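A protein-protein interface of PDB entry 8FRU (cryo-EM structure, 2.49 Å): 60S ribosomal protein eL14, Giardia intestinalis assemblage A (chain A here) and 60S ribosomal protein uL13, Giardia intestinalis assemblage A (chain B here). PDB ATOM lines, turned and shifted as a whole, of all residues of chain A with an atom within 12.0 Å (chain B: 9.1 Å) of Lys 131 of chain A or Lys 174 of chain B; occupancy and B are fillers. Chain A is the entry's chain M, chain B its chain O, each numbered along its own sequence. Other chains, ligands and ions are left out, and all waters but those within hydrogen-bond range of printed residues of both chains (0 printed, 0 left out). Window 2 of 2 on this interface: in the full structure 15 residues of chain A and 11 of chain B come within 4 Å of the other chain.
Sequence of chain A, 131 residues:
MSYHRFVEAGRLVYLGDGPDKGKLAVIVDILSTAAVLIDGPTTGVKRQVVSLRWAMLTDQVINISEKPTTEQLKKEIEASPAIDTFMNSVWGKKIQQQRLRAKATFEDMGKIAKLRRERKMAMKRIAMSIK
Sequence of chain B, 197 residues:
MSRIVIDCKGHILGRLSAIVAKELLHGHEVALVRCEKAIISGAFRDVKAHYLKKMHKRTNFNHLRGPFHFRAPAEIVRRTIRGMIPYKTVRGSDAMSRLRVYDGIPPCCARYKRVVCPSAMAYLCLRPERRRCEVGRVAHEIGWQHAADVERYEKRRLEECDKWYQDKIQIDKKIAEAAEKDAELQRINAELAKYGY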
ATOM      1  N   ALA A 122     -11.403  -7.210  -3.794  1.00  0.00           N
ATOM      2  CA  ALA A 122     -10.807  -8.403  -4.382  1.00  0.00           C
ATOM      3  C   ALA A 122     -10.370  -8.148  -5.818  1.00  0.00           C
ATOM      4  O   ALA A 122      -9.322  -8.638  -6.251  1.00  0.00           O
ATOM      5  CB  ALA A 122     -11.788  -9.571  -4.314  1.00  0.00           C
ATOM      6  N   MET A 123     -11.163  -7.390  -6.575  1.00  0.00           N
ATOM      7  CA  MET A 123     -10.790  -7.082  -7.952  1.00  0.00           C
ATOM      8  C   MET A 123      -9.501  -6.275  -8.010  1.00  0.00           C
ATOM      9  O   MET A 123      -8.640  -6.524  -8.860  1.00  0.00           O
ATOM     10  CB  MET A 123     -11.918  -6.320  -8.644  1.00  0.00           C
ATOM     11  CG  MET A 123     -12.229  -6.802 -10.045  1.00  0.00           C
ATOM     12  SD  MET A 123     -12.495  -8.578 -10.136  1.00  0.00           S
ATOM     13  CE  MET A 123     -13.156  -8.903  -8.507  1.00  0.00           C
ATOM     14  N   LYS A 124      -9.357  -5.292  -7.124  1.00  0.00           N
ATOM     15  CA  LYS A 124      -8.160  -4.459  -7.130  1.00  0.00           C
ATOM     16  C   LYS A 124      -6.915  -5.288  -6.840  1.00  0.00           C
ATOM     17  O   LYS A 124      -5.880  -5.131  -7.496  1.00  0.00           O
ATOM     18  CB  LYS A 124      -8.310  -3.331  -6.112  1.00  0.00           C
ATOM     19  CG  LYS A 124      -7.249  -2.260  -6.196  1.00  0.00           C
ATOM     20  CD  LYS A 124      -6.909  -1.752  -4.809  1.00  0.00           C
ATOM     21  CE  LYS A 124      -6.437  -0.308  -4.841  1.00  0.00           C
ATOM     22  NZ  LYS A 124      -6.534   0.314  -3.494  1.00  0.00           N
ATOM     23  N   ARG A 125      -6.997  -6.178  -5.853  1.00  0.00           N
ATOM     24  CA  ARG A 125      -5.851  -7.015  -5.522  1.00  0.00           C
ATOM     25  C   ARG A 125      -5.488  -7.943  -6.676  1.00  0.00           C
ATOM     26  O   ARG A 125      -4.305  -8.143  -6.972  1.00  0.00           O
ATOM     27  CB  ARG A 125      -6.146  -7.812  -4.254  1.00  0.00           C
ATOM     28  CG  ARG A 125      -5.034  -8.738  -3.826  1.00  0.00           C
ATOM     29  CD  ARG A 125      -5.570  -9.821  -2.920  1.00  0.00           C
ATOM     30  NE  ARG A 125      -5.968 -11.010  -3.662  1.00  0.00           N
ATOM     31  CZ  ARG A 125      -7.196 -11.506  -3.681  1.00  0.00           C
ATOM     32  NH1 ARG A 125      -8.188 -10.922  -3.029  1.00  0.00           N
ATOM     33  NH2 ARG A 125      -7.437 -12.617  -4.372  1.00  0.00           N
ATOM     34  N   ILE A 126      -6.490  -8.525  -7.335  1.00  0.00           N
ATOM     35  CA  ILE A 126      -6.212  -9.434  -8.444  1.00  0.00           C
ATOM     36  C   ILE A 126      -5.516  -8.701  -9.581  1.00  0.00           C
ATOM     37  O   ILE A 126      -4.521  -9.184 -10.133  1.00  0.00           O
ATOM     38  CB  ILE A 126      -7.508 -10.103  -8.930  1.00  0.00           C
ATOM     39  CG1 ILE A 126      -8.014 -11.099  -7.889  1.00  0.00           C
ATOM     40  CG2 ILE A 126      -7.276 -10.768 -10.268  1.00  0.00           C
ATOM     41  CD1 ILE A 126      -7.004 -12.153  -7.519  1.00  0.00           C
ATOM     42  N   ALA A 127      -6.024  -7.525  -9.950  1.00  0.00           N
ATOM     43  CA  ALA A 127      -5.442  -6.791 -11.067  1.00  0.00           C
ATOM     44  C   ALA A 127      -4.000  -6.398 -10.780  1.00  0.00           C
ATOM     45  O   ALA A 127      -3.138  -6.493 -11.659  1.00  0.00           O
ATOM     46  CB  ALA A 127      -6.283  -5.554 -11.380  1.00  0.00           C
ATOM     47  N   MET A 128      -3.718  -5.955  -9.557  1.00  0.00           N
ATOM     48  CA  MET A 128      -2.353  -5.575  -9.209  1.00  0.00           C
ATOM     49  C   MET A 128      -1.424  -6.784  -9.210  1.00  0.00           C
ATOM     50  O   MET A 128      -0.310  -6.724  -9.744  1.00  0.00           O
ATOM     51  CB  MET A 128      -2.336  -4.889  -7.847  1.00  0.00           C
ATOM     52  CG  MET A 128      -2.497  -3.384  -7.901  1.00  0.00           C
ATOM     53  SD  MET A 128      -2.976  -2.716  -6.298  1.00  0.00           S
ATOM     54  CE  MET A 128      -2.452  -4.038  -5.211  1.00  0.00           C
ATOM     55  N   SER A 129      -1.866  -7.896  -8.619  1.00  0.00           N
ATOM     56  CA  SER A 129      -0.980  -9.040  -8.427  1.00  0.00           C
ATOM     57  C   SER A 129      -0.474  -9.578  -9.757  1.00  0.00           C
ATOM     58  O   SER A 129       0.734  -9.744  -9.956  1.00  0.00           O
ATOM     59  CB  SER A 129      -1.708 -10.141  -7.660  1.00  0.00           C
ATOM     60  OG  SER A 129      -2.797 -10.640  -8.418  1.00  0.00           O
ATOM     61  N   ILE A 130      -1.388  -9.868 -10.676  1.00  0.00           N
ATOM     62  CA  ILE A 130      -1.061 -10.395 -11.993  1.00  0.00           C
ATOM     63  C   ILE A 130      -1.613  -9.432 -13.029  1.00  0.00           C
ATOM     64  O   ILE A 130      -2.816  -9.150 -13.038  1.00  0.00           O
ATOM     65  CB  ILE A 130      -1.644 -11.805 -12.201  1.00  0.00           C
ATOM     66  CG1 ILE A 130      -1.211 -12.735 -11.068  1.00  0.00           C
ATOM     67  CG2 ILE A 130      -1.228 -12.361 -13.554  1.00  0.00           C
ATOM     68  CD1 ILE A 130      -1.779 -14.129 -11.181  1.00  0.00           C
ATOM     69  N   LYS A 131      -0.745  -8.939 -13.900  1.00  0.00           N
ATOM     70  CA  LYS A 131      -1.165  -7.971 -14.903  1.00  0.00           C
ATOM     71  C   LYS A 131      -2.204  -8.557 -15.850  1.00  0.00           C
ATOM     72  O   LYS A 131      -2.789  -7.839 -16.658  1.00  0.00           O
ATOM     73  CB  LYS A 131       0.043  -7.465 -15.690  1.00  0.00           C
ATOM     74  CG  LYS A 131       1.134  -6.889 -14.811  1.00  0.00           C
ATOM     75  CD  LYS A 131       0.540  -5.912 -13.819  1.00  0.00           C
ATOM     76  CE  LYS A 131      -0.141  -4.759 -14.533  1.00  0.00           C
ATOM     77  NZ  LYS A 131      -0.825  -3.854 -13.569  1.00  0.00           N
ATOM     78  N   ASP B 167      -3.424  -3.051 -26.038  1.00  0.00           N
ATOM     79  CA  ASP B 167      -2.779  -3.410 -24.784  1.00  0.00           C
ATOM     80  C   ASP B 167      -3.820  -3.641 -23.702  1.00  0.00           C
ATOM     81  O   ASP B 167      -3.724  -4.596 -22.920  1.00  0.00           O
ATOM     82  CB  ASP B 167      -1.809  -2.309 -24.369  1.00  0.00           C
ATOM     83  CG  ASP B 167      -0.951  -1.844 -25.514  1.00  0.00           C
ATOM     84  OD1 ASP B 167      -1.036  -2.460 -26.597  1.00  0.00           O
ATOM     85  OD2 ASP B 167      -0.191  -0.870 -25.337  1.00  0.00           O
ATOM     86  N   LYS B 168      -4.827  -2.771 -23.651  1.00  0.00           N
ATOM     87  CA  LYS B 168      -5.924  -2.960 -22.717  1.00  0.00           C
ATOM     88  C   LYS B 168      -6.650  -4.268 -22.996  1.00  0.00           C
ATOM     89  O   LYS B 168      -7.046  -4.972 -22.066  1.00  0.00           O
ATOM     90  CB  LYS B 168      -6.884  -1.773 -22.799  1.00  0.00           C
ATOM     91  CG  LYS B 168      -7.656  -1.495 -21.523  1.00  0.00           C
ATOM     92  CD  LYS B 168      -9.135  -1.787 -21.690  1.00  0.00           C
ATOM     93  CE  LYS B 168      -9.949  -1.057 -20.636  1.00  0.00           C
ATOM     94  NZ  LYS B 168     -11.333  -1.589 -20.514  1.00  0.00           N
ATOM     95  N   ILE B 169      -6.816  -4.618 -24.271  1.00  0.00           N
ATOM     96  CA  ILE B 169      -7.504  -5.859 -24.617  1.00  0.00           C
ATOM     97  C   ILE B 169      -6.775  -7.053 -24.014  1.00  0.00           C
ATOM     98  O   ILE B 169      -7.369  -7.894 -23.322  1.00  0.00           O
ATOM     99  CB  ILE B 169      -7.612  -5.996 -26.145  1.00  0.00           C
ATOM    100  CG1 ILE B 169      -8.514  -4.911 -26.721  1.00  0.00           C
ATOM    101  CG2 ILE B 169      -8.131  -7.375 -26.526  1.00  0.00           C
ATOM    102  CD1 ILE B 169      -8.487  -4.856 -28.230  1.00  0.00           C
ATOM    103  N   GLN B 170      -5.469  -7.136 -24.259  1.00  0.00           N
ATOM    104  CA  GLN B 170      -4.710  -8.285 -23.770  1.00  0.00           C
ATOM    105  C   GLN B 170      -4.654  -8.307 -22.245  1.00  0.00           C
ATOM    106  O   GLN B 170      -4.827  -9.366 -21.621  1.00  0.00           O
ATOM    107  CB  GLN B 170      -3.304  -8.277 -24.362  1.00  0.00           C
ATOM    108  CG  GLN B 170      -3.291  -8.204 -25.875  1.00  0.00           C
ATOM    109  CD  GLN B 170      -3.724  -9.504 -26.520  1.00  0.00           C
ATOM    110  OE1 GLN B 170      -2.921 -10.416 -26.703  1.00  0.00           O
ATOM    111  NE2 GLN B 170      -5.004  -9.600 -26.857  1.00  0.00           N
ATOM    112  N   ILE B 171      -4.421  -7.150 -21.626  1.00  0.00           N
ATOM    113  CA  ILE B 171      -4.349  -7.104 -20.172  1.00  0.00           C
ATOM    114  C   ILE B 171      -5.681  -7.513 -19.565  1.00  0.00           C
ATOM    115  O   ILE B 171      -5.730  -8.216 -18.548  1.00  0.00           O
ATOM    116  CB  ILE B 171      -3.917  -5.701 -19.708  1.00  0.00           C
ATOM    117  CG1 ILE B 171      -2.509  -5.395 -20.213  1.00  0.00           C
ATOM    118  CG2 ILE B 171      -3.969  -5.603 -18.201  1.00  0.00           C
ATOM    119  CD1 ILE B 171      -1.583  -6.589 -20.193  1.00  0.00           C
ATOM    120  N   ASP B 172      -6.785  -7.077 -20.175  1.00  0.00           N
ATOM    121  CA  ASP B 172      -8.104  -7.432 -19.672  1.00  0.00           C
ATOM    122  C   ASP B 172      -8.341  -8.927 -19.776  1.00  0.00           C
ATOM    123  O   ASP B 172      -8.914  -9.535 -18.867  1.00  0.00           O
ATOM    124  CB  ASP B 172      -9.176  -6.667 -20.443  1.00  0.00           C
ATOM    125  CG  ASP B 172      -9.368  -5.261 -19.926  1.00  0.00           C
ATOM    126  OD1 ASP B 172      -8.839  -4.948 -18.839  1.00  0.00           O
ATOM    127  OD2 ASP B 172     -10.054  -4.470 -20.605  1.00  0.00           O
ATOM    128  N   LYS B 173      -7.919  -9.533 -20.885  1.00  0.00           N
ATOM    129  CA  LYS B 173      -8.051 -10.980 -21.023  1.00  0.00           C
ATOM    130  C   LYS B 173      -7.298 -11.702 -19.911  1.00  0.00           C
ATOM    131  O   LYS B 173      -7.827 -12.630 -19.278  1.00  0.00           O
ATOM    132  CB  LYS B 173      -7.541 -11.413 -22.395  1.00  0.00           C
ATOM    133  CG  LYS B 173      -7.665 -12.892 -22.672  1.00  0.00           C
ATOM    134  CD  LYS B 173      -7.568 -13.163 -24.161  1.00  0.00           C
ATOM    135  CE  LYS B 173      -6.569 -14.265 -24.462  1.00  0.00           C
ATOM    136  NZ  LYS B 173      -5.245 -13.719 -24.876  1.00  0.00           N
ATOM    137  N   LYS B 174      -6.059 -11.282 -19.653  1.00  0.00           N
ATOM    138  CA  LYS B 174      -5.277 -11.928 -18.600  1.00  0.00           C
ATOM    139  C   LYS B 174      -5.936 -11.754 -17.235  1.00  0.00           C
ATOM    140  O   LYS B 174      -6.000 -12.700 -16.438  1.00  0.00           O
ATOM    141  CB  LYS B 174      -3.858 -11.368 -18.581  1.00  0.00           C
ATOM    142  CG  LYS B 174      -3.070 -11.623 -19.852  1.00  0.00           C
ATOM    143  CD  LYS B 174      -1.663 -11.078 -19.735  1.00  0.00           C
ATOM    144  CE  LYS B 174      -1.148 -11.188 -18.309  1.00  0.00           C
ATOM    145  NZ  LYS B 174      -0.896 -12.596 -17.903  1.00  0.00           N
ATOM    146  N   ILE B 175      -6.422 -10.546 -16.944  1.00  0.00           N
ATOM    147  CA  ILE B 175      -7.056 -10.296 -15.654  1.00  0.00           C
ATOM    148  C   ILE B 175      -8.308 -11.143 -15.507  1.00  0.00           C
ATOM    149  O   ILE B 175      -8.600 -11.662 -14.424  1.00  0.00           O
ATOM    150  CB  ILE B 175      -7.370  -8.798 -15.490  1.00  0.00           C
ATOM    151  CG1 ILE B 175      -6.079  -7.983 -15.484  1.00  0.00           C
ATOM    152  CG2 ILE B 175      -8.147  -8.561 -14.208  1.00  0.00           C
ATOM    153  CD1 ILE B 175      -5.392  -7.950 -14.144  1.00  0.00           C
ATOM    154  N   ALA B 176      -9.075 -11.293 -16.587  1.00  0.00           N
ATOM    155  CA  ALA B 176     -10.270 -12.126 -16.526  1.00  0.00           C
ATOM    156  C   ALA B 176      -9.915 -13.575 -16.232  1.00  0.00           C
ATOM    157  O   ALA B 176     -10.574 -14.228 -15.413  1.00  0.00           O
ATOM    158  CB  ALA B 176     -11.055 -12.017 -17.832  1.00  0.00           C
ATOM    159  N   GLU B 177      -8.882 -14.105 -16.892  1.00  0.00           N
ATOM    160  CA  GLU B 177      -8.502 -15.490 -16.625  1.00  0.00           C
ATOM    161  C   GLU B 177      -8.045 -15.665 -15.181  1.00  0.00           C
ATOM    162  O   GLU B 177      -8.416 -16.641 -14.515  1.00  0.00           O
ATOM    163  CB  GLU B 177      -7.412 -15.952 -17.595  1.00  0.00           C
ATOM    164  CG  GLU B 177      -6.038 -15.383 -17.313  1.00  0.00           C
ATOM    165  CD  GLU B 177      -4.956 -16.014 -18.165  1.00  0.00           C
ATOM    166  OE1 GLU B 177      -4.672 -17.213 -17.972  1.00  0.00           O
ATOM    167  OE2 GLU B 177      -4.390 -15.309 -19.028  1.00  0.00           O
ATOM    168  N   ALA B 178      -7.246 -14.725 -14.674  1.00  0.00           N
ATOM    169  CA  ALA B 178      -6.792 -14.828 -13.291  1.00  0.00           C
ATOM    170  C   ALA B 178      -7.961 -14.755 -12.315  1.00  0.00           C
ATOM    171  O   ALA B 178      -7.998 -15.490 -11.321  1.00  0.00           O
ATOM    172  CB  ALA B 178      -5.769 -13.734 -12.985  1.00  0.00           C
ATOM    173  N   ALA B 179      -8.921 -13.863 -12.575  1.00  0.00           N
ATOM    174  CA  ALA B 179     -10.082 -13.743 -11.700  1.00  0.00           C
ATOM    175  C   ALA B 179     -10.920 -15.012 -11.719  1.00  0.00           C
ATOM    176  O   ALA B 179     -11.422 -15.449 -10.678  1.00  0.00           O
ATOM    177  CB  ALA B 179     -10.928 -12.539 -12.110  1.00  0.00           C
ATOM    178  N   GLU B 180     -11.095 -15.612 -12.896  1.00  0.00           N
ATOM    179  CA  GLU B 180     -11.809 -16.881 -12.961  1.00  0.00           C
ATOM    180  C   GLU B 180     -11.088 -17.947 -12.152  1.00  0.00           C
ATOM    181  O   GLU B 180     -11.719 -18.721 -11.423  1.00  0.00           O
ATOM    182  CB  GLU B 180     -11.969 -17.328 -14.412  1.00  0.00           C
ATOM    183  CG  GLU B 180     -12.396 -18.775 -14.563  1.00  0.00           C
ATOM    184  CD  GLU B 180     -11.628 -19.500 -15.653  1.00  0.00           C
ATOM    185  OE1 GLU B 180     -10.523 -19.038 -16.011  1.00  0.00           O
ATOM    186  OE2 GLU B 180     -12.128 -20.531 -16.150  1.00  0.00           O
ATOM    187  N   LYS B 181      -9.761 -17.999 -12.263  1.00  0.00           N
ATOM    188  CA  LYS B 181      -9.004 -19.006 -11.528  1.00  0.00           C
ATOM    189  C   LYS B 181      -9.126 -18.807 -10.020  1.00  0.00           C
ATOM    190  O   LYS B 181      -9.279 -19.779  -9.272  1.00  0.00           O
ATOM    191  CB  LYS B 181      -7.538 -18.975 -11.961  1.00  0.00           C
ATOM    192  CG  LYS B 181      -6.656 -20.038 -11.319  1.00  0.00           C
ATOM    193  CD  LYS B 181      -7.198 -21.449 -11.517  1.00  0.00           C
ATOM    194  CE  LYS B 181      -8.022 -21.581 -12.792  1.00  0.00           C
ATOM    195  NZ  LYS B 181      -7.179 -21.564 -14.016  1.00  0.00           N
ATOM    196  N   ASP B 182      -9.073 -17.560  -9.557  1.00  0.00           N
ATOM    197  CA  ASP B 182      -8.991 -17.296  -8.125  1.00  0.00           C
ATOM    198  C   ASP B 182     -10.203 -17.850  -7.382  1.00  0.00           C
ATOM    199  O   ASP B 182     -11.328 -17.839  -7.883  1.00  0.00           O
ATOM    200  CB  ASP B 182      -8.870 -15.799  -7.860  1.00  0.00           C
ATOM    201  CG  ASP B 182      -8.188 -15.498  -6.546  1.00  0.00           C
ATOM    202  OD1 ASP B 182      -8.874 -15.510  -5.503  1.00  0.00           O
ATOM    203  OD2 ASP B 182      -6.966 -15.253  -6.552  1.00  0.00           O
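OD1 of Asp 182 of chain B is in salt-bridge range of NH2 of Arg 125 of chain A, 3.4 Å away.
Ile 126 of chain A touches Asp 182 of chain B.
CA of Ala 127 of chain A touches CD1 of Ile 175 of chain B (3.3 Å).
Ile 175 of chain B touches Ile 130 of chain A.
Ile 171 of chain B touches Lys 131 of chain A (CG2 to O, 3.0 Å).
Lys 174 of chain B touches Lys 131 of chain A.
Lys 131 of chain A touches Ile 175 of chain B (O to CG1, 3.5 Å).
The backbone carbonyl oxygen (O) of Arg 125 of chain A sits at hydrogen-bond distance from the side-chain hydroxyl (OG) of Ser 129 of chain A, at 3.3 Å.
O of Ile 126 of chain A lies within hydrogen-bond range of OG of Ser 129 of chain A, 2.8 Å away.
Of the printed residues of chain B, Lys 131 of chain A touches Ile 171, Lys 174 and Ile 175.
Lys 174 of chain B touches just one residue of chain A: Lys 131.
No residue of chain A comes within 4 Å of Gln 170 of chain B.
No residue of chain A comes within 4 Å of Lys 173 of chain B.
Glu 177 of chain B touches none of the printed residues of chain A.
No residue of chain A comes within 4 Å of Ala 178 of chain B.
Printed residues of chain B within 4 Å of Ile 130 of chain A: Ile 175 (3.0 Å).
Of the printed residues of chain B, Ile 126 of chain A touches Asp 182 (3.2 Å).
Printed residues of chain B within 4 Å of Ala 127 of chain A: Ile 175 (3.3 Å).
Of the printed residues of chain B, Arg 125 of chain A touches Asp 182.
Of the printed residues of chain A, Asp 182 of chain B touches Arg 125 and Ile 126.
Ile 169 of chain B touches none of the printed residues of chain A.
Ala 179 of chain B touches none of the printed residues of chain A.
The nearest residue of chain B that does not touch Lys 131 of chain A is Asp 172 of chain B (5.4 Å).
The nearest residue of chain A that does not touch Lys 174 of chain B is Ile 130 of chain A (4.4 Å).
The nearest printed residue of chain A that does not touch Asp 182 of chain B is Ser 129 of chain A (6.5 Å).
Of the 10 printed residues of chain A, 5 touch a printed residue of chain B.
Hydrophobic or aromatic side chains of chain A within 4 Å of the printed part of chain B: Ile 126 and Ala 127.
Among the printed residues, 7 pairs touch across the chains.
Among the printed residues, Asp or Glu carboxylates within 4 Å of a Lys or Arg side-chain nitrogen of the other chain: Arg 125 of chain A with Asp 182 of chain B (3.4 Å).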
